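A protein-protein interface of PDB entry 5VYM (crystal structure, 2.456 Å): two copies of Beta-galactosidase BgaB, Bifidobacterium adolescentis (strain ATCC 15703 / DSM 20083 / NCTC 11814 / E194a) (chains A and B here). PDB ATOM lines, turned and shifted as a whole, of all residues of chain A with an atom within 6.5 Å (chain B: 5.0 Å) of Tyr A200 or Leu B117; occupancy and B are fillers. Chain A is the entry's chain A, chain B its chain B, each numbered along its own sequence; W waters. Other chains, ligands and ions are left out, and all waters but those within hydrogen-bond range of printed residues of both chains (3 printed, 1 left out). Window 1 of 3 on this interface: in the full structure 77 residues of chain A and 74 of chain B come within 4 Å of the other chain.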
ATOM      1  N   ALA A  85      17.111  29.286 -25.280  1.00  0.00           N
ATOM      2  CA  ALA A  85      18.386  28.764 -25.765  1.00  0.00           C
ATOM      3  C   ALA A  85      19.388  29.877 -26.044  1.00  0.00           C
ATOM      4  O   ALA A  85      20.594  29.687 -25.851  1.00  0.00           O
ATOM      5  CB  ALA A  85      18.166  27.923 -27.023  1.00  0.00           C
ATOM      6  N   ASP A 115       4.025  19.392 -27.940  1.00  0.00           N
ATOM      7  CA  ASP A 115       4.239  17.944 -27.999  1.00  0.00           C
ATOM      8  C   ASP A 115       5.478  17.539 -27.200  1.00  0.00           C
ATOM      9  O   ASP A 115       6.228  16.637 -27.580  1.00  0.00           O
ATOM     10  CB  ASP A 115       4.333  17.462 -29.451  1.00  0.00           C
ATOM     11  CG  ASP A 115       4.144  15.957 -29.588  1.00  0.00           C
ATOM     12  OD1 ASP A 115       3.878  15.286 -28.568  1.00  0.00           O
ATOM     13  OD2 ASP A 115       4.263  15.442 -30.722  1.00  0.00           O
ATOM     14  N   GLY A 116       5.699  18.223 -26.076  1.00  0.00           N
ATOM     15  CA  GLY A 116       6.808  17.925 -25.190  1.00  0.00           C
ATOM     16  C   GLY A 116       7.935  18.935 -25.202  1.00  0.00           C
ATOM     17  O   GLY A 116       8.886  18.779 -24.426  1.00  0.00           O
ATOM     18  N   LEU A 117       7.869  19.968 -26.046  1.00  0.00           N
ATOM     19  CA  LEU A 117       8.966  20.927 -26.113  1.00  0.00           C
ATOM     20  C   LEU A 117       9.011  21.810 -24.873  1.00  0.00           C
ATOM     21  O   LEU A 117      10.090  22.061 -24.324  1.00  0.00           O
ATOM     22  CB  LEU A 117       8.849  21.782 -27.373  1.00  0.00           C
ATOM     23  CG  LEU A 117      10.002  22.762 -27.592  1.00  0.00           C
ATOM     24  CD1 LEU A 117      11.329  22.019 -27.616  1.00  0.00           C
ATOM     25  CD2 LEU A 117       9.800  23.548 -28.878  1.00  0.00           C
ATOM     26  N   ARG A 119       7.657  21.051 -21.898  1.00  0.00           N
ATOM     27  CA  ARG A 119       8.006  20.120 -20.830  1.00  0.00           C
ATOM     28  C   ARG A 119       9.512  19.900 -20.746  1.00  0.00           C
ATOM     29  O   ARG A 119      10.090  19.886 -19.652  1.00  0.00           O
ATOM     30  CB  ARG A 119       7.275  18.799 -21.072  1.00  0.00           C
ATOM     31  CG  ARG A 119       7.479  17.725 -20.036  1.00  0.00           C
ATOM     32  CD  ARG A 119       6.956  16.415 -20.589  1.00  0.00           C
ATOM     33  NE  ARG A 119       5.703  16.616 -21.311  1.00  0.00           N
ATOM     34  CZ  ARG A 119       5.309  15.881 -22.346  1.00  0.00           C
ATOM     35  NH1 ARG A 119       6.074  14.894 -22.792  1.00  0.00           N
ATOM     36  NH2 ARG A 119       4.154  16.139 -22.941  1.00  0.00           N
ATOM     37  N   SER A 120      10.169  19.734 -21.897  1.00  0.00           N
ATOM     38  CA  SER A 120      11.609  19.503 -21.894  1.00  0.00           C
ATOM     39  C   SER A 120      12.385  20.749 -21.485  1.00  0.00           C
ATOM     40  O   SER A 120      13.448  20.635 -20.862  1.00  0.00           O
ATOM     41  CB  SER A 120      12.072  19.032 -23.270  1.00  0.00           C
ATOM     42  OG  SER A 120      12.139  20.113 -24.182  1.00  0.00           O
ATOM     43  N   MET A 121      11.885  21.939 -21.835  1.00  0.00           N
ATOM     44  CA  MET A 121      12.523  23.171 -21.381  1.00  0.00           C
ATOM     45  C   MET A 121      12.569  23.233 -19.861  1.00  0.00           C
ATOM     46  O   MET A 121      13.587  23.617 -19.275  1.00  0.00           O
ATOM     47  CB  MET A 121      11.778  24.392 -21.923  1.00  0.00           C
ATOM     48  CG  MET A 121      11.877  24.617 -23.415  1.00  0.00           C
ATOM     49  SD  MET A 121      10.873  26.042 -23.885  1.00  0.00           S
ATOM     50  CE  MET A 121      11.420  27.234 -22.663  1.00  0.00           C
ATOM     51  N   ASN A 198      17.485  19.495 -36.983  1.00  0.00           N
ATOM     52  CA  ASN A 198      16.697  20.473 -36.250  1.00  0.00           C
ATOM     53  C   ASN A 198      17.493  21.031 -35.073  1.00  0.00           C
ATOM     54  O   ASN A 198      18.118  20.255 -34.327  1.00  0.00           O
ATOM     55  CB  ASN A 198      15.396  19.836 -35.754  1.00  0.00           C
ATOM     56  CG  ASN A 198      14.482  20.829 -35.066  1.00  0.00           C
ATOM     57  OD1 ASN A 198      14.208  21.907 -35.593  1.00  0.00           O
ATOM     58  ND2 ASN A 198      14.009  20.471 -33.877  1.00  0.00           N
ATOM     59  N   PRO A 199      17.501  22.350 -34.879  1.00  0.00           N
ATOM     60  CA  PRO A 199      18.130  22.907 -33.676  1.00  0.00           C
ATOM     61  C   PRO A 199      17.321  22.569 -32.434  1.00  0.00           C
ATOM     62  O   PRO A 199      16.090  22.653 -32.430  1.00  0.00           O
ATOM     63  CB  PRO A 199      18.139  24.418 -33.940  1.00  0.00           C
ATOM     64  CG  PRO A 199      17.912  24.565 -35.411  1.00  0.00           C
ATOM     65  CD  PRO A 199      17.061  23.402 -35.807  1.00  0.00           C
ATOM     66  N   TYR A 200      18.027  22.181 -31.376  1.00  0.00           N
ATOM     67  CA  TYR A 200      17.401  21.884 -30.093  1.00  0.00           C
ATOM     68  C   TYR A 200      18.283  22.449 -28.994  1.00  0.00           C
ATOM     69  O   TYR A 200      19.417  21.993 -28.815  1.00  0.00           O
ATOM     70  CB  TYR A 200      17.195  20.378 -29.902  1.00  0.00           C
ATOM     71  CG  TYR A 200      16.528  20.039 -28.592  1.00  0.00           C
ATOM     72  CD1 TYR A 200      15.158  20.202 -28.425  1.00  0.00           C
ATOM     73  CD2 TYR A 200      17.269  19.567 -27.518  1.00  0.00           C
ATOM     74  CE1 TYR A 200      14.544  19.899 -27.226  1.00  0.00           C
ATOM     75  CE2 TYR A 200      16.664  19.261 -26.313  1.00  0.00           C
ATOM     76  CZ  TYR A 200      15.302  19.430 -26.174  1.00  0.00           C
ATOM     77  OH  TYR A 200      14.699  19.126 -24.977  1.00  0.00           O
ATOM     78  N   GLY A 201      17.761  23.425 -28.256  1.00  0.00           N
ATOM     79  CA  GLY A 201      18.593  24.135 -27.299  1.00  0.00           C
ATOM     80  C   GLY A 201      19.773  24.755 -28.018  1.00  0.00           C
ATOM     81  O   GLY A 201      19.625  25.397 -29.064  1.00  0.00           O
ATOM     82  N   SER A 202      20.967  24.551 -27.471  1.00  0.00           N
ATOM     83  CA  SER A 202      22.192  24.965 -28.138  1.00  0.00           C
ATOM     84  C   SER A 202      22.739  23.899 -29.077  1.00  0.00           C
ATOM     85  O   SER A 202      23.808  24.101 -29.662  1.00  0.00           O
ATOM     86  CB  SER A 202      23.259  25.335 -27.104  1.00  0.00           C
ATOM     87  OG  SER A 202      22.881  26.493 -26.383  1.00  0.00           O
ATOM     88  N   GLY A 203      22.035  22.781 -29.241  1.00  0.00           N
ATOM     89  CA  GLY A 203      22.526  21.690 -30.059  1.00  0.00           C
ATOM     90  C   GLY A 203      21.698  21.396 -31.291  1.00  0.00           C
ATOM     91  O   GLY A 203      21.060  22.293 -31.851  1.00  0.00           O
ATOM     92  N   GLU A 204      21.690  20.135 -31.716  1.00  0.00           N
ATOM     93  CA  GLU A 204      21.126  19.771 -33.007  1.00  0.00           C
ATOM     94  C   GLU A 204      20.747  18.296 -32.986  1.00  0.00           C
ATOM     95  O   GLU A 204      21.353  17.499 -32.267  1.00  0.00           O
ATOM     96  CB  GLU A 204      22.127  20.057 -34.129  1.00  0.00           C
ATOM     97  CG  GLU A 204      21.522  20.247 -35.501  1.00  0.00           C
ATOM     98  CD  GLU A 204      22.566  20.640 -36.524  1.00  0.00           C
ATOM     99  OE1 GLU A 204      23.763  20.373 -36.278  1.00  0.00           O
ATOM    100  OE2 GLU A 204      22.197  21.223 -37.566  1.00  0.00           O
ATOM    101  N   ALA A 205      19.742  17.945 -33.790  1.00  0.00           N
ATOM    102  CA  ALA A 205      19.237  16.576 -33.851  1.00  0.00           C
ATOM    103  C   ALA A 205      18.931  16.213 -35.295  1.00  0.00           C
ATOM    104  O   ALA A 205      18.089  16.854 -35.931  1.00  0.00           O
ATOM    105  CB  ALA A 205      17.988  16.408 -32.981  1.00  0.00           C
ATOM    106  N   THR B  77      16.288   8.798 -22.938  1.00  0.00           N
ATOM    107  CA  THR B  77      15.822   9.871 -23.811  1.00  0.00           C
ATOM    108  C   THR B  77      16.095  11.232 -23.181  1.00  0.00           C
ATOM    109  O   THR B  77      16.449  12.191 -23.877  1.00  0.00           O
ATOM    110  CB  THR B  77      14.330   9.702 -24.109  1.00  0.00           C
ATOM    111  OG1 THR B  77      14.087   8.385 -24.615  1.00  0.00           O
ATOM    112  CG2 THR B  77      13.874  10.716 -25.145  1.00  0.00           C
ATOM    113  N   GLN B  78      15.953  11.326 -21.856  1.00  0.00           N
ATOM    114  CA  GLN B  78      16.276  12.565 -21.157  1.00  0.00           C
ATOM    115  C   GLN B  78      17.768  12.867 -21.230  1.00  0.00           C
ATOM    116  O   GLN B  78      18.166  14.034 -21.331  1.00  0.00           O
ATOM    117  CB  GLN B  78      15.812  12.479 -19.702  1.00  0.00           C
ATOM    118  CG  GLN B  78      16.051  13.744 -18.892  1.00  0.00           C
ATOM    119  CD  GLN B  78      15.267  14.928 -19.416  1.00  0.00           C
ATOM    120  OE1 GLN B  78      14.070  14.826 -19.683  1.00  0.00           O
ATOM    121  NE2 GLN B  78      15.941  16.060 -19.576  1.00  0.00           N
ATOM    122  N   ALA B  81      18.355  14.480 -24.513  1.00  0.00           N
ATOM    123  CA  ALA B  81      17.851  15.849 -24.536  1.00  0.00           C
ATOM    124  C   ALA B  81      18.777  16.789 -23.776  1.00  0.00           C
ATOM    125  O   ALA B  81      19.065  17.897 -24.242  1.00  0.00           O
ATOM    126  CB  ALA B  81      16.438  15.901 -23.959  1.00  0.00           C
ATOM    127  N   ALA B  84      21.910  17.198 -25.948  1.00  0.00           N
ATOM    128  CA  ALA B  84      21.718  18.042 -27.122  1.00  0.00           C
ATOM    129  C   ALA B  84      21.463  19.493 -26.732  1.00  0.00           C
ATOM    130  O   ALA B  84      22.029  20.408 -27.339  1.00  0.00           O
ATOM    131  CB  ALA B  84      20.569  17.504 -27.974  1.00  0.00           C
ATOM    132  N   ALA B  85      20.621  19.724 -25.721  1.00  0.00           N
ATOM    133  CA  ALA B  85      20.289  21.090 -25.328  1.00  0.00           C
ATOM    134  C   ALA B  85      21.505  21.866 -24.844  1.00  0.00           C
ATOM    135  O   ALA B  85      21.484  23.101 -24.867  1.00  0.00           O
ATOM    136  CB  ALA B  85      19.212  21.086 -24.242  1.00  0.00           C
ATOM    137  N   ALA B 113       9.700   7.561 -28.147  1.00  0.00           N
ATOM    138  CA  ALA B 113      10.527   7.590 -26.945  1.00  0.00           C
ATOM    139  C   ALA B 113      10.447   8.948 -26.256  1.00  0.00           C
ATOM    140  O   ALA B 113      10.582   9.995 -26.896  1.00  0.00           O
ATOM    141  CB  ALA B 113      11.977   7.262 -27.295  1.00  0.00           C
ATOM    142  N   GLY B 114      10.218   8.924 -24.945  1.00  0.00           N
ATOM    143  CA  GLY B 114      10.151  10.140 -24.162  1.00  0.00           C
ATOM    144  C   GLY B 114       8.811  10.839 -24.159  1.00  0.00           C
ATOM    145  O   GLY B 114       8.730  11.975 -23.676  1.00  0.00           O
ATOM    146  N   ASP B 115       7.761  10.200 -24.680  1.00  0.00           N
ATOM    147  CA  ASP B 115       6.418  10.781 -24.729  1.00  0.00           C
ATOM    148  C   ASP B 115       6.435  12.139 -25.434  1.00  0.00           C
ATOM    149  O   ASP B 115       5.857  13.122 -24.965  1.00  0.00           O
ATOM    150  CB  ASP B 115       5.818  10.888 -23.322  1.00  0.00           C
ATOM    151  CG  ASP B 115       4.328  11.181 -23.341  1.00  0.00           C
ATOM    152  OD1 ASP B 115       3.575  10.415 -23.980  1.00  0.00           O
ATOM    153  OD2 ASP B 115       3.909  12.175 -22.709  1.00  0.00           O
ATOM    154  N   GLY B 116       7.117  12.186 -26.576  1.00  0.00           N
ATOM    155  CA  GLY B 116       7.252  13.398 -27.356  1.00  0.00           C
ATOM    156  C   GLY B 116       8.607  14.062 -27.256  1.00  0.00           C
ATOM    157  O   GLY B 116       8.906  14.943 -28.072  1.00  0.00           O
ATOM    158  N   LEU B 117       9.436  13.666 -26.288  1.00  0.00           N
ATOM    159  CA  LEU B 117      10.743  14.293 -26.125  1.00  0.00           C
ATOM    160  C   LEU B 117      11.608  14.087 -27.364  1.00  0.00           C
ATOM    161  O   LEU B 117      12.235  15.031 -27.861  1.00  0.00           O
ATOM    162  CB  LEU B 117      11.432  13.738 -24.877  1.00  0.00           C
ATOM    163  CG  LEU B 117      12.806  14.316 -24.535  1.00  0.00           C
ATOM    164  CD1 LEU B 117      12.755  15.829 -24.538  1.00  0.00           C
ATOM    165  CD2 LEU B 117      13.277  13.804 -23.185  1.00  0.00           C
ATOM    166  N   LEU B 118      11.646  12.859 -27.884  1.00  0.00           N
ATOM    167  CA  LEU B 118      12.439  12.602 -29.081  1.00  0.00           C
ATOM    168  C   LEU B 118      11.872  13.342 -30.287  1.00  0.00           C
ATOM    169  O   LEU B 118      12.629  13.896 -31.093  1.00  0.00           O
ATOM    170  CB  LEU B 118      12.513  11.098 -29.346  1.00  0.00           C
ATOM    171  CG  LEU B 118      13.532  10.644 -30.393  1.00  0.00           C
ATOM    172  CD1 LEU B 118      14.913  11.202 -30.080  1.00  0.00           C
ATOM    173  CD2 LEU B 118      13.571   9.125 -30.474  1.00  0.00           C
ATOM    174  N   ARG B 119      10.543  13.367 -30.425  1.00  0.00           N
ATOM    175  CA  ARG B 119       9.928  14.147 -31.494  1.00  0.00           C
ATOM    176  C   ARG B 119      10.291  15.621 -31.378  1.00  0.00           C
ATOM    177  O   ARG B 119      10.599  16.274 -32.383  1.00  0.00           O
ATOM    178  CB  ARG B 119       8.409  13.977 -31.470  1.00  0.00           C
ATOM    179  CG  ARG B 119       7.928  12.586 -31.818  1.00  0.00           C
ATOM    180  CD  ARG B 119       6.425  12.565 -32.049  1.00  0.00           C
ATOM    181  NE  ARG B 119       5.666  12.926 -30.854  1.00  0.00           N
ATOM    182  CZ  ARG B 119       5.226  12.051 -29.954  1.00  0.00           C
ATOM    183  NH1 ARG B 119       5.474  10.758 -30.108  1.00  0.00           N
ATOM    184  NH2 ARG B 119       4.538  12.467 -28.900  1.00  0.00           N
ATOM    185  N   SER B 120      10.261  16.162 -30.156  1.00  0.00           N
ATOM    186  CA  SER B 120      10.569  17.575 -29.961  1.00  0.00           C
ATOM    187  C   SER B 120      12.007  17.887 -30.354  1.00  0.00           C
ATOM    188  O   SER B 120      12.274  18.907 -30.999  1.00  0.00           O
ATOM    189  CB  SER B 120      10.312  17.975 -28.508  1.00  0.00           C
ATOM    190  OG  SER B 120       8.946  17.808 -28.171  1.00  0.00           O
ATOM    191  N   MET B 121      12.949  17.021 -29.969  1.00  0.00           N
ATOM    192  CA  MET B 121      14.338  17.206 -30.378  1.00  0.00           C
ATOM    193  C   MET B 121      14.466  17.205 -31.896  1.00  0.00           C
ATOM    194  O   MET B 121      15.099  18.091 -32.481  1.00  0.00           O
ATOM    195  CB  MET B 121      15.218  16.108 -29.773  1.00  0.00           C
ATOM    196  CG  MET B 121      15.263  16.076 -28.253  1.00  0.00           C
ATOM    197  SD  MET B 121      16.153  14.625 -27.652  1.00  0.00           S
ATOM    198  CE  MET B 121      17.652  14.746 -28.618  1.00  0.00           C
ATOM    199  N   TYR B 200      18.577  25.592 -20.097  1.00  0.00           N
ATOM    200  CA  TYR B 200      18.203  25.206 -21.455  1.00  0.00           C
ATOM    201  C   TYR B 200      19.035  26.042 -22.414  1.00  0.00           C
ATOM    202  O   TYR B 200      18.783  27.240 -22.575  1.00  0.00           O
ATOM    203  CB  TYR B 200      16.707  25.411 -21.699  1.00  0.00           C
ATOM    204  CG  TYR B 200      16.213  24.853 -23.013  1.00  0.00           C
ATOM    205  CD1 TYR B 200      15.836  23.519 -23.124  1.00  0.00           C
ATOM    206  CD2 TYR B 200      16.117  25.657 -24.141  1.00  0.00           C
ATOM    207  CE1 TYR B 200      15.382  23.004 -24.323  1.00  0.00           C
ATOM    208  CE2 TYR B 200      15.665  25.149 -25.345  1.00  0.00           C
ATOM    209  CZ  TYR B 200      15.299  23.820 -25.430  1.00  0.00           C
ATOM    210  OH  TYR B 200      14.845  23.305 -26.624  1.00  0.00           O
HETATM  211  O   HOH W   1       8.556  13.736 -21.291  1.00  0.00           O
HETATM  212  O   HOH W   2      11.860  21.659 -32.274  1.00  0.00           O
HETATM  213  O   HOH W   3      14.924  24.584 -28.936  1.00  0.00           O
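The side-chain carboxylate (OD2) of Asp A115 lies within salt-bridge range of the guanidinium group (NE) of Arg B119, 2.9 Å away. The backbone carbonyl oxygen (O) of Ala B85 is in hydrogen-bond range of the backbone NH (N) of Ser A202 (3.0 Å). The backbone NH of Leu A117 is in hydrogen-bond range of the side-chain hydroxyl of Ser B120, 3.2 Å away. The side-chain hydroxyl (OG) of Ser B120 lies within hydrogen-bond range of the backbone carbonyl oxygen (O) of Asp A115 (3.0 Å). The backbone carbonyl oxygen (O) of Ala B84 sits close to the backbone carbonyl oxygen (O) of Tyr A200 (3.4 Å). NH1 of Arg A119 is in salt-bridge range of OD2 of Asp B115 (3.5 Å). The backbone carbonyl oxygen (O) of Asp A115 lies close to the backbone carbonyl oxygen (O) of Gly B116, 3.2 Å away. The backbone NH of Gly A203 sits at hydrogen-bond distance from the backbone carbonyl oxygen of Ala B84 (3.0 Å). The side-chain amide nitrogen (ND2) of Asn A198 lies within hydrogen-bond range of the backbone carbonyl oxygen (O) of Met B121 (3.0 Å). N of Gly A201 sits at hydrogen-bond distance from OH of Tyr B200, 3.3 Å away.
Printed residues of chain B within 4 Å of Leu A117: Ser B120 (3.2 Å) and Tyr B200 (3.9 Å). Tyr A200 touches just these residues of chain B: Ala B81 (3.5 Å), Ala B84 (3.4 Å), Ala B85 (3.7 Å), Leu B117 (3.9 Å), Met B121 (3.7 Å) and Tyr B200 (3.5 Å). Gln B78 touches none of the printed residues of chain A. Leu B117 touches just these residues of chain A: Ser A120 and Tyr A200. Of the printed residues of chain A, Tyr B200 touches Ala A85, Leu A117, Met A121, Tyr A200 and Gly A201. The nearest residue of chain A that does not touch Leu B117 is Asp A115 (4.6 Å). The nearest printed residue of chain B that does not touch Met A121 is Leu B117 (6.7 Å).
The backbone carbonyl oxygen of Gly B116 is in hydrogen-bond range of the side-chain hydroxyl of Ser B120 (2.9 Å). The backbone carbonyl oxygen (O) of Asn A198 is in hydrogen-bond range of the backbone NH (N) of Ala A205 (2.9 Å). O of Leu A117 is in hydrogen-bond range of OG of Ser A120, 2.8 Å away. OG of Ser A120 lies within hydrogen-bond range of OH of Tyr A200, at 2.9 Å.
Water W3 bridges the side-chain hydroxyl of Tyr B200 (2.6 Å) and the backbone NH of Gly A201 (3.1 Å). Water W2 bridges the side-chain amide nitrogen of Asn A198 (2.9 Å) and the backbone carbonyl oxygen of Ser B120 (3.1 Å). Water W1 bridges the backbone carbonyl oxygen of Gly B114 (3.0 Å) and the guanidinium group of Arg A119 (3.1 Å).
Along chain B the printed residues that touch a printed residue of chain A span positions 81 to 200. Of the 15 printed residues of chain A, 13 touch a printed residue of chain B. Among the printed residues, 24 pairs touch across the chains.
Ala A85 touches Tyr B200, and with the chains exchanged Tyr A200 touches Ala B85. Asp A115 touches Ser B120, but with the chains exchanged Ser A120 does not touch Asp B115 (8.5 Å). Gly A116 touches Ser B120, but with the chains exchanged Ser A120 does not touch Gly B116 (7.1 Å). Tyr A200 touches its own counterpart, Tyr B200. Positions printed for both chains: 85, 115, 116, 117, 119, 120, 121 and 200. Of the 24 pairs that touch across the chains among the printed residues, 11 have their exchanged pair printed and touching as well.
CA of Ala A85 touches O of Tyr B200, 3.6 Å away. Tyr B200 touches Leu A117. CB of Ser A120 touches CD1 of Leu B117, at 3.5 Å. Tyr B200 touches Met A121 (CD1 to CA, 3.8 Å). O of Ser B120 touches ND2 of Asn A198 (3.7 Å). Tyr A200 touches Ala B85 (O to CA, 3.7 Å). Tyr A200 touches Leu B117. Tyr A200 touches Tyr B200 (CE1 to OH, 3.5 Å). CA of Gly A201 touches O of Ala B85, at 3.9 Å. Ala B84 touches Ser A202.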
